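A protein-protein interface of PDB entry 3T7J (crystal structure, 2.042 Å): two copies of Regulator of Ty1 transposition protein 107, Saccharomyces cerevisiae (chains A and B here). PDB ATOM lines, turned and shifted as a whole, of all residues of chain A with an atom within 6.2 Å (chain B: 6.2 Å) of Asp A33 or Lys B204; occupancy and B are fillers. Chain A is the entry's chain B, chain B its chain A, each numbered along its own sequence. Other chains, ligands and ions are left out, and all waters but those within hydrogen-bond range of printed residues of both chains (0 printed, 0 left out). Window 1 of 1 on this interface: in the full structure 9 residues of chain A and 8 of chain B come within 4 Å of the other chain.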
ATOM      1  N   CYS A  30      30.380  -4.306   8.824  1.00  0.00           N
ATOM      2  CA  CYS A  30      29.163  -4.082   9.597  1.00  0.00           C
ATOM      3  C   CYS A  30      29.018  -2.607   9.984  1.00  0.00           C
ATOM      4  O   CYS A  30      29.975  -1.831   9.889  1.00  0.00           O
ATOM      5  CB  CYS A  30      29.135  -4.980  10.843  1.00  0.00           C
ATOM      6  SG  CYS A  30      30.520  -4.722  11.998  1.00  0.00           S
ATOM      7  N   PHE A  31      27.810  -2.228  10.396  1.00  0.00           N
ATOM      8  CA  PHE A  31      27.497  -0.845  10.756  1.00  0.00           C
ATOM      9  C   PHE A  31      28.051   0.166   9.770  1.00  0.00           C
ATOM     10  O   PHE A  31      28.692   1.138  10.177  1.00  0.00           O
ATOM     11  CB  PHE A  31      28.045  -0.519  12.144  1.00  0.00           C
ATOM     12  CG  PHE A  31      27.568  -1.445  13.214  1.00  0.00           C
ATOM     13  CD1 PHE A  31      26.222  -1.490  13.561  1.00  0.00           C
ATOM     14  CD2 PHE A  31      28.460  -2.266  13.885  1.00  0.00           C
ATOM     15  CE1 PHE A  31      25.780  -2.346  14.551  1.00  0.00           C
ATOM     16  CE2 PHE A  31      28.015  -3.125  14.898  1.00  0.00           C
ATOM     17  CZ  PHE A  31      26.680  -3.165  15.223  1.00  0.00           C
ATOM     18  N   HIS A  32      27.800  -0.044   8.479  1.00  0.00           N
ATOM     19  CA  HIS A  32      28.439   0.767   7.436  1.00  0.00           C
ATOM     20  C   HIS A  32      28.055   2.250   7.493  1.00  0.00           C
ATOM     21  O   HIS A  32      28.876   3.125   7.215  1.00  0.00           O
ATOM     22  CB  HIS A  32      28.180   0.180   6.041  1.00  0.00           C
ATOM     23  CG  HIS A  32      26.834   0.511   5.475  1.00  0.00           C
ATOM     24  ND1 HIS A  32      26.668   1.375   4.411  1.00  0.00           N
ATOM     25  CD2 HIS A  32      25.592   0.087   5.808  1.00  0.00           C
ATOM     26  CE1 HIS A  32      25.386   1.470   4.118  1.00  0.00           C
ATOM     27  NE2 HIS A  32      24.708   0.700   4.953  1.00  0.00           N
ATOM     28  N   ASP A  33      26.809   2.523   7.862  1.00  0.00           N
ATOM     29  CA  ASP A  33      26.328   3.896   8.028  1.00  0.00           C
ATOM     30  C   ASP A  33      26.617   4.463   9.427  1.00  0.00           C
ATOM     31  O   ASP A  33      26.613   5.683   9.626  1.00  0.00           O
ATOM     32  CB  ASP A  33      24.826   3.967   7.735  1.00  0.00           C
ATOM     33  CG  ASP A  33      24.040   2.890   8.460  1.00  0.00           C
ATOM     34  OD1 ASP A  33      24.623   1.828   8.781  1.00  0.00           O
ATOM     35  OD2 ASP A  33      22.834   3.103   8.702  1.00  0.00           O
ATOM     36  N   GLY A  34      26.854   3.581  10.394  1.00  0.00           N
ATOM     37  CA  GLY A  34      27.225   4.014  11.731  1.00  0.00           C
ATOM     38  C   GLY A  34      26.103   4.046  12.753  1.00  0.00           C
ATOM     39  O   GLY A  34      25.094   3.347  12.620  1.00  0.00           O
ATOM     40  N   PHE A  35      26.290   4.867  13.785  1.00  0.00           N
ATOM     41  CA  PHE A  35      25.340   4.965  14.894  1.00  0.00           C
ATOM     42  C   PHE A  35      24.848   6.397  15.087  1.00  0.00           C
ATOM     43  O   PHE A  35      25.588   7.351  14.856  1.00  0.00           O
ATOM     44  CB  PHE A  35      25.997   4.485  16.192  1.00  0.00           C
ATOM     45  CG  PHE A  35      26.618   3.124  16.083  1.00  0.00           C
ATOM     46  CD1 PHE A  35      25.939   2.003  16.520  1.00  0.00           C
ATOM     47  CD2 PHE A  35      27.879   2.964  15.527  1.00  0.00           C
ATOM     48  CE1 PHE A  35      26.501   0.746  16.410  1.00  0.00           C
ATOM     49  CE2 PHE A  35      28.448   1.704  15.409  1.00  0.00           C
ATOM     50  CZ  PHE A  35      27.757   0.598  15.851  1.00  0.00           C
ATOM     51  N   ILE A  40      25.766   6.455  20.307  1.00  0.00           N
ATOM     52  CA  ILE A  40      27.192   6.653  20.540  1.00  0.00           C
ATOM     53  C   ILE A  40      27.460   7.033  21.991  1.00  0.00           C
ATOM     54  O   ILE A  40      28.452   6.598  22.580  1.00  0.00           O
ATOM     55  CB  ILE A  40      27.785   7.731  19.645  1.00  0.00           C
ATOM     56  CG1 ILE A  40      27.974   7.198  18.226  1.00  0.00           C
ATOM     57  CG2 ILE A  40      29.128   8.207  20.211  1.00  0.00           C
ATOM     58  CD1 ILE A  40      28.654   8.180  17.314  1.00  0.00           C
ATOM     59  N   ASP A  52      36.197   5.606  13.873  1.00  0.00           N
ATOM     60  CA  ASP A  52      36.006   5.471  12.421  1.00  0.00           C
ATOM     61  C   ASP A  52      37.197   4.792  11.779  1.00  0.00           C
ATOM     62  O   ASP A  52      37.050   3.901  10.945  1.00  0.00           O
ATOM     63  CB  ASP A  52      35.874   6.842  11.761  1.00  0.00           C
ATOM     64  CG  ASP A  52      34.601   7.559  12.136  1.00  0.00           C
ATOM     65  OD1 ASP A  52      33.558   6.887  12.311  1.00  0.00           O
ATOM     66  OD2 ASP A  52      34.652   8.804  12.237  1.00  0.00           O
ATOM     67  N   VAL B 147      32.883  12.963   0.062  1.00  0.00           N
ATOM     68  CA  VAL B 147      33.581  12.989   1.352  1.00  0.00           C
ATOM     69  C   VAL B 147      34.806  12.065   1.338  1.00  0.00           C
ATOM     70  O   VAL B 147      34.709  10.883   0.975  1.00  0.00           O
ATOM     71  CB  VAL B 147      32.650  12.599   2.504  1.00  0.00           C
ATOM     72  CG1 VAL B 147      31.527  13.612   2.643  1.00  0.00           C
ATOM     73  CG2 VAL B 147      32.086  11.201   2.269  1.00  0.00           C
ATOM     74  N   ASP B 149      36.272  10.253   3.209  1.00  0.00           N
ATOM     75  CA  ASP B 149      36.241   8.953   3.881  1.00  0.00           C
ATOM     76  C   ASP B 149      35.406   7.922   3.123  1.00  0.00           C
ATOM     77  O   ASP B 149      34.891   6.968   3.708  1.00  0.00           O
ATOM     78  CB  ASP B 149      35.797   9.064   5.352  1.00  0.00           C
ATOM     79  CG  ASP B 149      34.343   9.491   5.514  1.00  0.00           C
ATOM     80  OD1 ASP B 149      34.049  10.199   6.497  1.00  0.00           O
ATOM     81  OD2 ASP B 149      33.487   9.115   4.690  1.00  0.00           O
ATOM     82  N   LYS B 175      36.436  16.570   8.803  1.00  0.00           N
ATOM     83  CA  LYS B 175      35.427  17.597   8.995  1.00  0.00           C
ATOM     84  C   LYS B 175      36.030  18.999   9.020  1.00  0.00           C
ATOM     85  O   LYS B 175      35.690  19.821   9.874  1.00  0.00           O
ATOM     86  CB  LYS B 175      34.637  17.312  10.278  1.00  0.00           C
ATOM     87  CG  LYS B 175      35.427  16.565  11.356  1.00  0.00           C
ATOM     88  CD  LYS B 175      35.607  15.078  11.031  1.00  0.00           C
ATOM     89  CE  LYS B 175      34.631  14.193  11.804  1.00  0.00           C
ATOM     90  NZ  LYS B 175      33.210  14.556  11.560  1.00  0.00           N
ATOM     91  N   VAL B 202      28.021  11.001   0.514  1.00  0.00           N
ATOM     92  CA  VAL B 202      28.527  10.922   1.885  1.00  0.00           C
ATOM     93  C   VAL B 202      28.459   9.504   2.423  1.00  0.00           C
ATOM     94  O   VAL B 202      27.720   8.670   1.896  1.00  0.00           O
ATOM     95  CB  VAL B 202      27.772  11.887   2.842  1.00  0.00           C
ATOM     96  CG1 VAL B 202      27.802  13.306   2.310  1.00  0.00           C
ATOM     97  CG2 VAL B 202      26.343  11.433   3.061  1.00  0.00           C
ATOM     98  N   THR B 203      29.239   9.228   3.463  1.00  0.00           N
ATOM     99  CA  THR B 203      29.315   7.881   4.015  1.00  0.00           C
ATOM    100  C   THR B 203      28.642   7.773   5.387  1.00  0.00           C
ATOM    101  O   THR B 203      27.912   6.824   5.651  1.00  0.00           O
ATOM    102  CB  THR B 203      30.775   7.411   4.131  1.00  0.00           C
ATOM    103  OG1 THR B 203      31.409   7.483   2.846  1.00  0.00           O
ATOM    104  CG2 THR B 203      30.835   5.979   4.634  1.00  0.00           C
ATOM    105  N   LYS B 204      28.887   8.741   6.258  1.00  0.00           N
ATOM    106  CA  LYS B 204      28.306   8.693   7.598  1.00  0.00           C
ATOM    107  C   LYS B 204      27.076   9.584   7.718  1.00  0.00           C
ATOM    108  O   LYS B 204      27.115  10.766   7.388  1.00  0.00           O
ATOM    109  CB  LYS B 204      29.338   9.054   8.670  1.00  0.00           C
ATOM    110  CG  LYS B 204      28.832   8.785  10.088  1.00  0.00           C
ATOM    111  CD  LYS B 204      29.968   8.541  11.071  1.00  0.00           C
ATOM    112  CE  LYS B 204      30.644   9.840  11.482  1.00  0.00           C
ATOM    113  NZ  LYS B 204      31.746   9.605  12.456  1.00  0.00           N
ATOM    114  N   ALA B 205      25.985   9.007   8.206  1.00  0.00           N
ATOM    115  CA  ALA B 205      24.707   9.711   8.266  1.00  0.00           C
ATOM    116  C   ALA B 205      24.704  10.952   9.179  1.00  0.00           C
ATOM    117  O   ALA B 205      23.654  11.558   9.409  1.00  0.00           O
ATOM    118  CB  ALA B 205      23.583   8.741   8.642  1.00  0.00           C
ATOM    119  N   SER B 206      25.879  11.335   9.678  1.00  0.00           N
ATOM    120  CA  SER B 206      26.024  12.549  10.476  1.00  0.00           C
ATOM    121  C   SER B 206      26.748  13.620   9.679  1.00  0.00           C
ATOM    122  O   SER B 206      26.832  14.781  10.098  1.00  0.00           O
ATOM    123  CB  SER B 206      26.805  12.268  11.760  1.00  0.00           C
ATOM    124  OG  SER B 206      28.003  13.034  11.786  1.00  0.00           O
ATOM    125  N   GLN B 207      27.306  13.223   8.543  1.00  0.00           N
ATOM    126  CA  GLN B 207      27.845  14.181   7.592  1.00  0.00           C
ATOM    127  C   GLN B 207      26.668  14.890   6.916  1.00  0.00           C
ATOM    128  O   GLN B 207      26.814  15.976   6.353  1.00  0.00           O
ATOM    129  CB  GLN B 207      28.721  13.476   6.546  1.00  0.00           C
ATOM    130  CG  GLN B 207      29.928  12.746   7.125  1.00  0.00           C
ATOM    131  CD  GLN B 207      30.792  12.078   6.067  1.00  0.00           C
ATOM    132  OE1 GLN B 207      30.309  11.282   5.241  1.00  0.00           O
ATOM    133  NE2 GLN B 207      32.086  12.388   6.092  1.00  0.00           N
ATOM    134  N   VAL B 208      25.500  14.260   6.974  1.00  0.00           N
ATOM    135  CA  VAL B 208      24.307  14.820   6.370  1.00  0.00           C
ATOM    136  C   VAL B 208      23.916  16.078   7.131  1.00  0.00           C
ATOM    137  O   VAL B 208      23.731  17.144   6.540  1.00  0.00           O
ATOM    138  CB  VAL B 208      23.155  13.817   6.423  1.00  0.00           C
ATOM    139  CG1 VAL B 208      21.866  14.441   5.891  1.00  0.00           C
ATOM    140  CG2 VAL B 208      23.517  12.548   5.664  1.00  0.00           C
ATOM    141  N   GLU B 228      24.227   7.997  -0.840  1.00  0.00           N
ATOM    142  CA  GLU B 228      25.261   7.035  -0.507  1.00  0.00           C
ATOM    143  C   GLU B 228      25.865   6.525  -1.810  1.00  0.00           C
ATOM    144  O   GLU B 228      25.252   6.612  -2.870  1.00  0.00           O
ATOM    145  CB  GLU B 228      24.673   5.858   0.290  1.00  0.00           C
ATOM    146  CG  GLU B 228      24.115   6.241   1.659  1.00  0.00           C
ATOM    147  CD  GLU B 228      23.378   5.096   2.353  1.00  0.00           C
ATOM    148  OE1 GLU B 228      22.335   4.649   1.832  1.00  0.00           O
ATOM    149  OE2 GLU B 228      23.838   4.648   3.426  1.00  0.00           O
ATOM    150  N   LEU B 250      19.922  10.023   1.193  1.00  0.00           N
ATOM    151  CA  LEU B 250      20.003  10.365   2.595  1.00  0.00           C
ATOM    152  C   LEU B 250      19.243  11.642   2.898  1.00  0.00           C
ATOM    153  O   LEU B 250      18.764  11.841   4.013  1.00  0.00           O
ATOM    154  CB  LEU B 250      21.459  10.510   3.003  1.00  0.00           C
ATOM    155  CG  LEU B 250      22.245   9.211   2.891  1.00  0.00           C
ATOM    156  CD1 LEU B 250      23.664   9.456   3.353  1.00  0.00           C
ATOM    157  CD2 LEU B 250      21.582   8.124   3.738  1.00  0.00           C
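The backbone NH (N) of Lys B204 sits at hydrogen-bond distance from the side-chain amide oxygen (OE1) of Gln B207, 3.1 Å away.
Asp A33 touches just these residues of chain B: Lys B204 (3.8 Å) and Ala B205 (3.7 Å). Of the printed residues of chain A, Lys B204 touches Asp A33 (3.8 Å) and Asp A52 (3.0 Å). Printed residues of chain A within 4 Å of Glu B228: His A32. Printed residues of chain A within 4 Å of Ala B205: Asp A33 (3.7 Å). Printed residues of chain B within 4 Å of Asp A52: Lys B204. Of the printed residues of chain B, His A32 touches Glu B228. The nearest residue of chain B that does not touch Asp A33 is Thr B203 (4.1 Å).
Printed residues of chain B that touch a printed residue of chain A: Lys B204, Ala B205 and Glu B228. Among the printed residues, Asp or Glu carboxylates within 4 Å of a Lys or Arg side-chain nitrogen of the other chain: Asp A52 with Lys B204 (3.0 Å).
NZ of Lys B204 is in salt-bridge range of OD2 of Asp A52.
Among the printed residues, pairs that only touch across the chains: His A32 with Glu B228 (3.6 Å), Asp A33 with Lys B204 (3.8 Å) and Asp A33 with Ala B205 (3.7 Å).
No position is printed for both chains. Of the 4 pairs that touch across the chains among the printed residues, none has its exchanged pair printed and touching as well.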
